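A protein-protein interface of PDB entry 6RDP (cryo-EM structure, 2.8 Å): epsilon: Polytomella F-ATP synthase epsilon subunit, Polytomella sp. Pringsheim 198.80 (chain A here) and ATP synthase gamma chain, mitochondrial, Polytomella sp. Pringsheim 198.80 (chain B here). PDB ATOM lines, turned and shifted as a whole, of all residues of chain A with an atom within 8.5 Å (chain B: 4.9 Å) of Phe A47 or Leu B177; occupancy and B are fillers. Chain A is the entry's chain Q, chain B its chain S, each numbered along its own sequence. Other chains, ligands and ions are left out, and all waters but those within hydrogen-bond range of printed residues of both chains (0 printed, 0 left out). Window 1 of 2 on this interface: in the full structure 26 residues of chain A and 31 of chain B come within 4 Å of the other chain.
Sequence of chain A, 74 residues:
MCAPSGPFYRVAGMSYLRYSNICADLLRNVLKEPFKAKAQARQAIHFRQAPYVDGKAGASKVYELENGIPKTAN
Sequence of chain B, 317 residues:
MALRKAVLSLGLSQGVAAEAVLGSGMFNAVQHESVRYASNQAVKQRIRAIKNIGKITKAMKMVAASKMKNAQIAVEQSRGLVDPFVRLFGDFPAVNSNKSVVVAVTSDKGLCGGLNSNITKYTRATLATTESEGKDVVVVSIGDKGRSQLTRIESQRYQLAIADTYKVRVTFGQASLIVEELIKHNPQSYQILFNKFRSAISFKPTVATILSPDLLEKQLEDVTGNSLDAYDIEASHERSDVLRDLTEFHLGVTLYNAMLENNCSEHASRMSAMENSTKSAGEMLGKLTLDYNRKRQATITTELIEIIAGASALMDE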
ATOM      1  N   SER A  15      -6.206 -22.868  -8.531  1.00  0.00           N
ATOM      2  CA  SER A  15      -4.779 -23.100  -8.677  1.00  0.00           C
ATOM      3  C   SER A  15      -4.505 -24.598  -8.754  1.00  0.00           C
ATOM      4  O   SER A  15      -5.388 -25.432  -8.528  1.00  0.00           O
ATOM      5  CB  SER A  15      -4.016 -22.471  -7.518  1.00  0.00           C
ATOM      6  OG  SER A  15      -4.302 -23.145  -6.307  1.00  0.00           O
ATOM      7  N   LEU A  17      -2.253 -26.172  -6.783  1.00  0.00           N
ATOM      8  CA  LEU A  17      -1.985 -26.679  -5.443  1.00  0.00           C
ATOM      9  C   LEU A  17      -3.270 -27.028  -4.718  1.00  0.00           C
ATOM     10  O   LEU A  17      -3.317 -28.011  -3.969  1.00  0.00           O
ATOM     11  CB  LEU A  17      -1.195 -25.653  -4.647  1.00  0.00           C
ATOM     12  CG  LEU A  17       0.309 -25.872  -4.635  1.00  0.00           C
ATOM     13  CD1 LEU A  17       0.913 -24.899  -3.670  1.00  0.00           C
ATOM     14  CD2 LEU A  17       0.660 -27.302  -4.255  1.00  0.00           C
ATOM     15  N   ARG A  18      -4.334 -26.270  -4.971  1.00  0.00           N
ATOM     16  CA  ARG A  18      -5.620 -26.591  -4.370  1.00  0.00           C
ATOM     17  C   ARG A  18      -6.191 -27.877  -4.942  1.00  0.00           C
ATOM     18  O   ARG A  18      -6.754 -28.684  -4.204  1.00  0.00           O
ATOM     19  CB  ARG A  18      -6.600 -25.448  -4.576  1.00  0.00           C
ATOM     20  CG  ARG A  18      -7.751 -25.501  -3.608  1.00  0.00           C
ATOM     21  CD  ARG A  18      -8.600 -24.265  -3.720  1.00  0.00           C
ATOM     22  NE  ARG A  18      -8.070 -23.138  -2.973  1.00  0.00           N
ATOM     23  CZ  ARG A  18      -8.402 -22.870  -1.718  1.00  0.00           C
ATOM     24  NH1 ARG A  18      -9.255 -23.655  -1.077  1.00  0.00           N
ATOM     25  NH2 ARG A  18      -7.881 -21.819  -1.107  1.00  0.00           N
ATOM     26  N   ASN A  21      -4.090 -30.794  -3.588  1.00  0.00           N
ATOM     27  CA  ASN A  21      -4.391 -31.041  -2.187  1.00  0.00           C
ATOM     28  C   ASN A  21      -5.804 -31.571  -1.993  1.00  0.00           C
ATOM     29  O   ASN A  21      -6.046 -32.317  -1.046  1.00  0.00           O
ATOM     30  CB  ASN A  21      -4.173 -29.770  -1.381  1.00  0.00           C
ATOM     31  CG  ASN A  21      -2.759 -29.650  -0.888  1.00  0.00           C
ATOM     32  OD1 ASN A  21      -2.325 -30.410  -0.026  1.00  0.00           O
ATOM     33  ND2 ASN A  21      -2.014 -28.722  -1.460  1.00  0.00           N
ATOM     34  N   ALA A  44      -4.423 -30.907   8.808  1.00  0.00           N
ATOM     35  CA  ALA A  44      -5.024 -29.767   9.478  1.00  0.00           C
ATOM     36  C   ALA A  44      -4.413 -28.461   8.998  1.00  0.00           C
ATOM     37  O   ALA A  44      -3.197 -28.348   8.839  1.00  0.00           O
ATOM     38  CB  ALA A  44      -4.850 -29.891  10.990  1.00  0.00           C
ATOM     39  N   ILE A  45      -5.263 -27.466   8.782  1.00  0.00           N
ATOM     40  CA  ILE A  45      -4.826 -26.139   8.378  1.00  0.00           C
ATOM     41  C   ILE A  45      -5.246 -25.176   9.475  1.00  0.00           C
ATOM     42  O   ILE A  45      -6.416 -24.782   9.554  1.00  0.00           O
ATOM     43  CB  ILE A  45      -5.412 -25.723   7.028  1.00  0.00           C
ATOM     44  CG1 ILE A  45      -4.979 -26.701   5.937  1.00  0.00           C
ATOM     45  CG2 ILE A  45      -4.971 -24.337   6.676  1.00  0.00           C
ATOM     46  CD1 ILE A  45      -5.473 -26.335   4.561  1.00  0.00           C
ATOM     47  N   HIS A  46      -4.300 -24.804  10.330  1.00  0.00           N
ATOM     48  CA  HIS A  46      -4.530 -23.829  11.392  1.00  0.00           C
ATOM     49  C   HIS A  46      -3.493 -22.732  11.223  1.00  0.00           C
ATOM     50  O   HIS A  46      -2.329 -22.938  11.569  1.00  0.00           O
ATOM     51  CB  HIS A  46      -4.413 -24.454  12.773  1.00  0.00           C
ATOM     52  CG  HIS A  46      -5.412 -25.529  13.046  1.00  0.00           C
ATOM     53  ND1 HIS A  46      -5.082 -26.867  13.049  1.00  0.00           N
ATOM     54  CD2 HIS A  46      -6.732 -25.465  13.339  1.00  0.00           C
ATOM     55  CE1 HIS A  46      -6.157 -27.581  13.336  1.00  0.00           C
ATOM     56  NE2 HIS A  46      -7.171 -26.754  13.512  1.00  0.00           N
ATOM     57  N   PHE A  47      -3.902 -21.589  10.690  1.00  0.00           N
ATOM     58  CA  PHE A  47      -3.072 -20.393  10.694  1.00  0.00           C
ATOM     59  C   PHE A  47      -3.987 -19.188  10.548  1.00  0.00           C
ATOM     60  O   PHE A  47      -5.215 -19.311  10.596  1.00  0.00           O
ATOM     61  CB  PHE A  47      -1.987 -20.444   9.607  1.00  0.00           C
ATOM     62  CG  PHE A  47      -2.489 -20.242   8.205  1.00  0.00           C
ATOM     63  CD1 PHE A  47      -3.171 -21.244   7.538  1.00  0.00           C
ATOM     64  CD2 PHE A  47      -2.229 -19.062   7.535  1.00  0.00           C
ATOM     65  CE1 PHE A  47      -3.602 -21.056   6.251  1.00  0.00           C
ATOM     66  CE2 PHE A  47      -2.661 -18.871   6.243  1.00  0.00           C
ATOM     67  CZ  PHE A  47      -3.348 -19.871   5.602  1.00  0.00           C
ATOM     68  N   ARG A  48      -3.394 -18.014  10.396  1.00  0.00           N
ATOM     69  CA  ARG A  48      -4.161 -16.808  10.154  1.00  0.00           C
ATOM     70  C   ARG A  48      -3.353 -15.935   9.217  1.00  0.00           C
ATOM     71  O   ARG A  48      -2.154 -16.146   9.025  1.00  0.00           O
ATOM     72  CB  ARG A  48      -4.462 -16.053  11.449  1.00  0.00           C
ATOM     73  CG  ARG A  48      -3.252 -15.310  11.994  1.00  0.00           C
ATOM     74  CD  ARG A  48      -3.490 -14.660  13.333  1.00  0.00           C
ATOM     75  NE  ARG A  48      -2.289 -13.958  13.763  1.00  0.00           N
ATOM     76  CZ  ARG A  48      -2.126 -13.411  14.960  1.00  0.00           C
ATOM     77  NH1 ARG A  48      -0.990 -12.794  15.252  1.00  0.00           N
ATOM     78  NH2 ARG A  48      -3.086 -13.498  15.868  1.00  0.00           N
ATOM     79  N   GLN A  49      -4.020 -14.953   8.627  1.00  0.00           N
ATOM     80  CA  GLN A  49      -3.330 -13.951   7.835  1.00  0.00           C
ATOM     81  C   GLN A  49      -4.033 -12.617   7.987  1.00  0.00           C
ATOM     82  O   GLN A  49      -5.157 -12.532   8.482  1.00  0.00           O
ATOM     83  CB  GLN A  49      -3.255 -14.327   6.354  1.00  0.00           C
ATOM     84  CG  GLN A  49      -4.602 -14.536   5.713  1.00  0.00           C
ATOM     85  CD  GLN A  49      -4.514 -14.681   4.212  1.00  0.00           C
ATOM     86  OE1 GLN A  49      -3.487 -14.383   3.608  1.00  0.00           O
ATOM     87  NE2 GLN A  49      -5.592 -15.156   3.602  1.00  0.00           N
ATOM     88  N   ALA A  50      -3.343 -11.576   7.555  1.00  0.00           N
ATOM     89  CA  ALA A  50      -3.873 -10.226   7.546  1.00  0.00           C
ATOM     90  C   ALA A  50      -3.131  -9.417   6.494  1.00  0.00           C
ATOM     91  O   ALA A  50      -1.898  -9.344   6.533  1.00  0.00           O
ATOM     92  CB  ALA A  50      -3.741  -9.575   8.922  1.00  0.00           C
ATOM     93  N   SER A  60      -8.278  -9.000   9.398  1.00  0.00           N
ATOM     94  CA  SER A  60      -7.733 -10.313   9.704  1.00  0.00           C
ATOM     95  C   SER A  60      -8.543 -11.397   9.012  1.00  0.00           C
ATOM     96  O   SER A  60      -9.721 -11.216   8.695  1.00  0.00           O
ATOM     97  CB  SER A  60      -7.703 -10.578  11.215  1.00  0.00           C
ATOM     98  OG  SER A  60      -7.225 -11.882  11.488  1.00  0.00           O
ATOM     99  N   LYS A  61      -7.886 -12.532   8.795  1.00  0.00           N
ATOM    100  CA  LYS A  61      -8.475 -13.670   8.102  1.00  0.00           C
ATOM    101  C   LYS A  61      -7.938 -14.922   8.771  1.00  0.00           C
ATOM    102  O   LYS A  61      -6.735 -15.188   8.706  1.00  0.00           O
ATOM    103  CB  LYS A  61      -8.119 -13.639   6.615  1.00  0.00           C
ATOM    104  CG  LYS A  61      -8.457 -14.904   5.851  1.00  0.00           C
ATOM    105  CD  LYS A  61      -9.922 -14.951   5.476  1.00  0.00           C
ATOM    106  CE  LYS A  61     -10.218 -16.120   4.553  1.00  0.00           C
ATOM    107  NZ  LYS A  61      -9.528 -15.990   3.242  1.00  0.00           N
ATOM    108  N   VAL A  62      -8.815 -15.683   9.410  1.00  0.00           N
ATOM    109  CA  VAL A  62      -8.400 -16.741  10.317  1.00  0.00           C
ATOM    110  C   VAL A  62      -8.848 -18.089   9.765  1.00  0.00           C
ATOM    111  O   VAL A  62      -9.978 -18.243   9.295  1.00  0.00           O
ATOM    112  CB  VAL A  62      -8.966 -16.469  11.731  1.00  0.00           C
ATOM    113  CG1 VAL A  62      -8.830 -17.665  12.656  1.00  0.00           C
ATOM    114  CG2 VAL A  62      -8.276 -15.256  12.337  1.00  0.00           C
ATOM    115  N   TYR A  63      -7.947 -19.071   9.832  1.00  0.00           N
ATOM    116  CA  TYR A  63      -8.188 -20.426   9.364  1.00  0.00           C
ATOM    117  C   TYR A  63      -8.109 -21.365  10.554  1.00  0.00           C
ATOM    118  O   TYR A  63      -7.190 -21.271  11.369  1.00  0.00           O
ATOM    119  CB  TYR A  63      -7.163 -20.848   8.306  1.00  0.00           C
ATOM    120  CG  TYR A  63      -7.274 -20.128   6.983  1.00  0.00           C
ATOM    121  CD1 TYR A  63      -6.776 -18.839   6.822  1.00  0.00           C
ATOM    122  CD2 TYR A  63      -7.853 -20.745   5.890  1.00  0.00           C
ATOM    123  CE1 TYR A  63      -6.874 -18.185   5.613  1.00  0.00           C
ATOM    124  CE2 TYR A  63      -7.955 -20.102   4.680  1.00  0.00           C
ATOM    125  CZ  TYR A  63      -7.465 -18.825   4.545  1.00  0.00           C
ATOM    126  OH  TYR A  63      -7.571 -18.193   3.331  1.00  0.00           O
ATOM    127  N   GLU A  64      -9.087 -22.257  10.667  1.00  0.00           N
ATOM    128  CA  GLU A  64      -9.208 -23.150  11.815  1.00  0.00           C
ATOM    129  C   GLU A  64      -9.435 -24.576  11.345  1.00  0.00           C
ATOM    130  O   GLU A  64      -9.990 -25.407  12.070  1.00  0.00           O
ATOM    131  CB  GLU A  64     -10.353 -22.724  12.739  1.00  0.00           C
ATOM    132  CG  GLU A  64     -10.412 -21.245  13.116  1.00  0.00           C
ATOM    133  CD  GLU A  64     -11.226 -20.413  12.146  1.00  0.00           C
ATOM    134  OE1 GLU A  64     -11.402 -20.841  10.987  1.00  0.00           O
ATOM    135  OE2 GLU A  64     -11.695 -19.330  12.546  1.00  0.00           O
ATOM    136  N   LEU A  65      -8.992 -24.881  10.133  1.00  0.00           N
ATOM    137  CA  LEU A  65      -9.490 -26.039   9.409  1.00  0.00           C
ATOM    138  C   LEU A  65      -8.781 -27.310   9.846  1.00  0.00           C
ATOM    139  O   LEU A  65      -7.576 -27.463   9.639  1.00  0.00           O
ATOM    140  CB  LEU A  65      -9.316 -25.838   7.907  1.00  0.00           C
ATOM    141  CG  LEU A  65     -10.290 -24.862   7.254  1.00  0.00           C
ATOM    142  CD1 LEU A  65      -9.784 -23.433   7.250  1.00  0.00           C
ATOM    143  CD2 LEU A  65     -10.607 -25.317   5.865  1.00  0.00           C
ATOM    144  N   GLY A  68      -9.076 -30.287   6.293  1.00  0.00           N
ATOM    145  CA  GLY A  68      -8.276 -30.229   5.095  1.00  0.00           C
ATOM    146  C   GLY A  68      -8.406 -28.874   4.440  1.00  0.00           C
ATOM    147  O   GLY A  68      -8.679 -27.866   5.097  1.00  0.00           O
ATOM    148  N   ILE A  69      -8.198 -28.850   3.130  1.00  0.00           N
ATOM    149  CA  ILE A  69      -8.277 -27.624   2.342  1.00  0.00           C
ATOM    150  C   ILE A  69      -9.768 -27.391   2.109  1.00  0.00           C
ATOM    151  O   ILE A  69     -10.545 -28.356   2.167  1.00  0.00           O
ATOM    152  CB  ILE A  69      -7.437 -27.767   1.053  1.00  0.00           C
ATOM    153  CG1 ILE A  69      -6.906 -26.425   0.539  1.00  0.00           C
ATOM    154  CG2 ILE A  69      -8.199 -28.482  -0.046  1.00  0.00           C
ATOM    155  CD1 ILE A  69      -5.645 -26.535  -0.279  1.00  0.00           C
ATOM    156  N   PRO A  70     -10.244 -26.153   1.940  1.00  0.00           N
ATOM    157  CA  PRO A  70     -11.662 -25.964   1.590  1.00  0.00           C
ATOM    158  C   PRO A  70     -11.940 -26.420   0.165  1.00  0.00           C
ATOM    159  O   PRO A  70     -11.325 -25.933  -0.785  1.00  0.00           O
ATOM    160  CB  PRO A  70     -11.880 -24.453   1.747  1.00  0.00           C
ATOM    161  CG  PRO A  70     -10.726 -23.947   2.485  1.00  0.00           C
ATOM    162  CD  PRO A  70      -9.592 -24.872   2.262  1.00  0.00           C
ATOM    163  N   ASN A  74     -12.296 -20.481  -3.458  1.00  0.00           N
ATOM    164  CA  ASN A  74     -11.344 -19.683  -2.698  1.00  0.00           C
ATOM    165  C   ASN A  74     -11.741 -18.209  -2.669  1.00  0.00           C
ATOM    166  O   ASN A  74     -12.410 -17.756  -1.739  1.00  0.00           O
ATOM    167  CB  ASN A  74      -9.943 -19.846  -3.291  1.00  0.00           C
ATOM    168  CG  ASN A  74      -8.887 -19.091  -2.520  1.00  0.00           C
ATOM    169  OD1 ASN A  74      -8.950 -18.983  -1.294  1.00  0.00           O
ATOM    170  ND2 ASN A  74      -7.892 -18.575  -3.233  1.00  0.00           N
ATOM    171  N   ILE B 162       1.491 -13.568   7.715  1.00  0.00           N
ATOM    172  CA  ILE B 162       0.989 -14.883   8.080  1.00  0.00           C
ATOM    173  C   ILE B 162       1.521 -15.203   9.463  1.00  0.00           C
ATOM    174  O   ILE B 162       2.722 -15.072   9.720  1.00  0.00           O
ATOM    175  CB  ILE B 162       1.407 -15.954   7.061  1.00  0.00           C
ATOM    176  CG1 ILE B 162       0.916 -15.592   5.663  1.00  0.00           C
ATOM    177  CG2 ILE B 162       0.871 -17.301   7.462  1.00  0.00           C
ATOM    178  CD1 ILE B 162       2.004 -15.118   4.753  1.00  0.00           C
ATOM    179  N   ALA B 163       0.635 -15.595  10.366  1.00  0.00           N
ATOM    180  CA  ALA B 163       1.033 -15.850  11.733  1.00  0.00           C
ATOM    181  C   ALA B 163       0.190 -16.999  12.259  1.00  0.00           C
ATOM    182  O   ALA B 163      -0.670 -17.523  11.546  1.00  0.00           O
ATOM    183  CB  ALA B 163       0.892 -14.578  12.568  1.00  0.00           C
ATOM    184  N   ASP B 164       0.443 -17.378  13.515  1.00  0.00           N
ATOM    185  CA  ASP B 164      -0.161 -18.538  14.181  1.00  0.00           C
ATOM    186  C   ASP B 164       0.021 -19.821  13.383  1.00  0.00           C
ATOM    187  O   ASP B 164      -0.863 -20.678  13.352  1.00  0.00           O
ATOM    188  CB  ASP B 164      -1.642 -18.312  14.503  1.00  0.00           C
ATOM    189  CG  ASP B 164      -1.849 -17.383  15.682  1.00  0.00           C
ATOM    190  OD1 ASP B 164      -0.930 -17.267  16.521  1.00  0.00           O
ATOM    191  OD2 ASP B 164      -2.945 -16.798  15.793  1.00  0.00           O
ATOM    192  N   THR B 165       1.176 -19.964  12.749  1.00  0.00           N
ATOM    193  CA  THR B 165       1.421 -21.073  11.846  1.00  0.00           C
ATOM    194  C   THR B 165       1.998 -22.302  12.530  1.00  0.00           C
ATOM    195  O   THR B 165       1.766 -23.419  12.067  1.00  0.00           O
ATOM    196  CB  THR B 165       2.337 -20.617  10.712  1.00  0.00           C
ATOM    197  OG1 THR B 165       2.704 -21.752   9.922  1.00  0.00           O
ATOM    198  CG2 THR B 165       3.552 -19.911  11.233  1.00  0.00           C
ATOM    199  N   GLY B 173      -0.979 -28.490   3.235  1.00  0.00           N
ATOM    200  CA  GLY B 173      -2.134 -27.722   2.801  1.00  0.00           C
ATOM    201  C   GLY B 173      -2.064 -26.286   3.275  1.00  0.00           C
ATOM    202  O   GLY B 173      -2.485 -25.363   2.574  1.00  0.00           O
ATOM    203  N   GLN B 174      -1.472 -26.082   4.449  1.00  0.00           N
ATOM    204  CA  GLN B 174      -1.253 -24.748   4.987  1.00  0.00           C
ATOM    205  C   GLN B 174      -0.271 -23.955   4.140  1.00  0.00           C
ATOM    206  O   GLN B 174      -0.535 -22.800   3.787  1.00  0.00           O
ATOM    207  CB  GLN B 174      -0.727 -24.886   6.400  1.00  0.00           C
ATOM    208  CG  GLN B 174      -0.417 -23.611   7.056  1.00  0.00           C
ATOM    209  CD  GLN B 174       0.209 -23.845   8.382  1.00  0.00           C
ATOM    210  OE1 GLN B 174       0.521 -24.975   8.743  1.00  0.00           O
ATOM    211  NE2 GLN B 174       0.378 -22.790   9.134  1.00  0.00           N
ATOM    212  N   ALA B 175       0.865 -24.568   3.796  1.00  0.00           N
ATOM    213  CA  ALA B 175       1.832 -23.928   2.915  1.00  0.00           C
ATOM    214  C   ALA B 175       1.269 -23.731   1.520  1.00  0.00           C
ATOM    215  O   ALA B 175       1.644 -22.780   0.832  1.00  0.00           O
ATOM    216  CB  ALA B 175       3.104 -24.757   2.848  1.00  0.00           C
ATOM    217  N   SER B 176       0.342 -24.593   1.109  1.00  0.00           N
ATOM    218  CA  SER B 176      -0.351 -24.415  -0.157  1.00  0.00           C
ATOM    219  C   SER B 176      -1.240 -23.184  -0.135  1.00  0.00           C
ATOM    220  O   SER B 176      -1.282 -22.436  -1.111  1.00  0.00           O
ATOM    221  CB  SER B 176      -1.178 -25.653  -0.468  1.00  0.00           C
ATOM    222  OG  SER B 176      -0.406 -26.830  -0.326  1.00  0.00           O
ATOM    223  N   LEU B 177      -1.960 -22.959   0.967  1.00  0.00           N
ATOM    224  CA  LEU B 177      -2.794 -21.762   1.068  1.00  0.00           C
ATOM    225  C   LEU B 177      -1.955 -20.494   1.143  1.00  0.00           C
ATOM    226  O   LEU B 177      -2.332 -19.457   0.581  1.00  0.00           O
ATOM    227  CB  LEU B 177      -3.710 -21.854   2.280  1.00  0.00           C
ATOM    228  CG  LEU B 177      -4.745 -22.968   2.264  1.00  0.00           C
ATOM    229  CD1 LEU B 177      -5.740 -22.767   3.384  1.00  0.00           C
ATOM    230  CD2 LEU B 177      -5.451 -23.001   0.935  1.00  0.00           C
ATOM    231  N   ILE B 178      -0.815 -20.558   1.828  1.00  0.00           N
ATOM    232  CA  ILE B 178       0.078 -19.403   1.871  1.00  0.00           C
ATOM    233  C   ILE B 178       0.674 -19.138   0.491  1.00  0.00           C
ATOM    234  O   ILE B 178       0.815 -17.982   0.069  1.00  0.00           O
ATOM    235  CB  ILE B 178       1.154 -19.615   2.948  1.00  0.00           C
ATOM    236  CG1 ILE B 178       0.482 -19.780   4.297  1.00  0.00           C
ATOM    237  CG2 ILE B 178       2.057 -18.426   3.052  1.00  0.00           C
ATOM    238  CD1 ILE B 178       1.352 -20.404   5.323  1.00  0.00           C
ATOM    239  N   VAL B 179       0.957 -20.203  -0.267  1.00  0.00           N
ATOM    240  CA  VAL B 179       1.396 -20.049  -1.649  1.00  0.00           C
ATOM    241  C   VAL B 179       0.293 -19.470  -2.523  1.00  0.00           C
ATOM    242  O   VAL B 179       0.570 -18.671  -3.422  1.00  0.00           O
ATOM    243  CB  VAL B 179       1.863 -21.393  -2.199  1.00  0.00           C
ATOM    244  N   GLU B 180      -0.962 -19.847  -2.257  1.00  0.00           N
ATOM    245  CA  GLU B 180      -2.099 -19.297  -2.994  1.00  0.00           C
ATOM    246  C   GLU B 180      -2.218 -17.793  -2.794  1.00  0.00           C
ATOM    247  O   GLU B 180      -2.337 -17.034  -3.763  1.00  0.00           O
ATOM    248  CB  GLU B 180      -3.388 -19.967  -2.537  1.00  0.00           C
ATOM    249  CG  GLU B 180      -3.655 -21.315  -3.122  1.00  0.00           C
ATOM    250  CD  GLU B 180      -5.130 -21.540  -3.352  1.00  0.00           C
ATOM    251  OE1 GLU B 180      -5.591 -22.681  -3.163  1.00  0.00           O
ATOM    252  OE2 GLU B 180      -5.827 -20.574  -3.729  1.00  0.00           O
ATOM    253  N   GLU B 181      -2.176 -17.346  -1.542  1.00  0.00           N
ATOM    254  CA  GLU B 181      -2.219 -15.916  -1.262  1.00  0.00           C
ATOM    255  C   GLU B 181      -0.950 -15.178  -1.664  1.00  0.00           C
ATOM    256  O   GLU B 181      -0.991 -13.952  -1.794  1.00  0.00           O
ATOM    257  CB  GLU B 181      -2.538 -15.679   0.216  1.00  0.00           C
ATOM    258  CG  GLU B 181      -4.041 -15.555   0.554  1.00  0.00           C
ATOM    259  CD  GLU B 181      -4.856 -16.851   0.562  1.00  0.00           C
ATOM    260  OE1 GLU B 181      -4.540 -17.821  -0.154  1.00  0.00           O
ATOM    261  OE2 GLU B 181      -5.855 -16.891   1.305  1.00  0.00           O
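Leu B177 touches Arg A18. Gly B173 touches Ile A45 (C to CD1, 3.6 Å). N of Gln B174 touches CG1 of Ile A45 (3.9 Å). CG2 of Ile A45 touches CD1 of Leu B177 (3.7 Å). Gln B174 touches His A46. CD2 of Phe A47 touches CG2 of Ile B162, 3.6 Å away. Ala B163 touches Phe A47. CB of Phe A47 touches NE2 of Gln B174, at 3.4 Å. Phe A47 touches Leu B177 (CZ to CB, 3.9 Å). CD1 of Leu B177 touches CE2 of Tyr A63 (3.7 Å).
The side-chain hydroxyl (OG) of Ser A15 is in hydrogen-bond range of the backbone NH (N) of Arg A18, at 3.4 Å. The guanidinium group (NH1) of Arg A18 sits at hydrogen-bond distance from the backbone carbonyl oxygen (O) of Pro A70, 3.1 Å away. The guanidinium group of Arg A18 is in hydrogen-bond range of the side-chain amide oxygen of Asn A74 (3.0 Å). The backbone NH of Tyr A63 lies within hydrogen-bond range of the backbone carbonyl oxygen of Phe A47, 2.8 Å away. The backbone carbonyl oxygen (O) of Lys A61 sits at hydrogen-bond distance from the backbone NH (N) of Gln A49 (2.7 Å). The side-chain hydroxyl (OG1) of Thr B165 lies within hydrogen-bond range of the side-chain amide nitrogen (NE2) of Gln B174, 2.7 Å away.
Of the printed residues of chain B, Asn A21 touches Gly B173 and Ser B176. Ala A44 touches none of the printed residues of chain B. Of the printed residues of chain B, Ile A45 touches Gly B173 (3.6 Å), Gln B174 (3.9 Å) and Leu B177 (3.7 Å). Of the printed residues of chain B, Phe A47 touches Ile B162, Ala B163, Asp B164, Gln B174, Leu B177 and Ile B178. Glu A64 touches none of the printed residues of chain B. Of the printed residues of chain A, Gln B174 touches Ile A45 (3.9 Å), His A46 (3.6 Å) and Phe A47 (3.4 Å). Ser B176 touches just these residues of chain A: Leu A17 (3.8 Å) and Asn A21 (2.7 Å). Of the printed residues of chain A, Ile B178 touches Phe A47 (3.8 Å). Of the printed residues of chain A, Glu B180 touches Ser A15 (3.4 Å), Arg A18 (2.5 Å) and Asn A74 (2.9 Å). The nearest residue of chain B that does not touch Phe A47 is Thr B165 (4.1 Å). The nearest residue of chain A that does not touch Leu B177 is Pro A70 (4.5 Å).
Hydrophobic or aromatic side chains of chain B within 4 Å of the printed part of chain A: Ile B162, Ala B163, Leu B177, Ile B178 and Val B179. Hydrophobic or aromatic side chains of chain A that line the printed part of chain B: Leu A17, Ile A45, Phe A47, Tyr A63 and Ile A69. Among the printed residues, 26 pairs touch across the chains.
OG of Ser A15 lies within hydrogen-bond range of OE1 of Glu B180, 3.4 Å away. The guanidinium group (NE) of Arg A18 is in salt-bridge range of the side-chain carboxylate (OE1) of Glu B180, at 2.5 Å. OG of Ser B176 lies within hydrogen-bond range of ND2 of Asn A21 (2.7 Å). The backbone NH (N) of Arg A48 is in hydrogen-bond range of the backbone carbonyl oxygen (O) of Ala B163 (3.0 Å). NH2 of Arg A48 is in salt-bridge range of OD2 of Asp B164, at 3.3 Å. The side-chain amide nitrogen (NE2) of Gln A49 is in hydrogen-bond range of the side-chain carboxylate (OE2) of Glu B181 (2.9 Å). OE2 of Glu B181 is in hydrogen-bond range of OH of Tyr A63, at 3.0 Å. ND2 of Asn A74 sits at hydrogen-bond distance from OE2 of Glu B180 (2.9 Å). The backbone carbonyl oxygen (O) of His A46 sits close to the backbone carbonyl oxygen (O) of Asp B164, 3.2 Å away.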
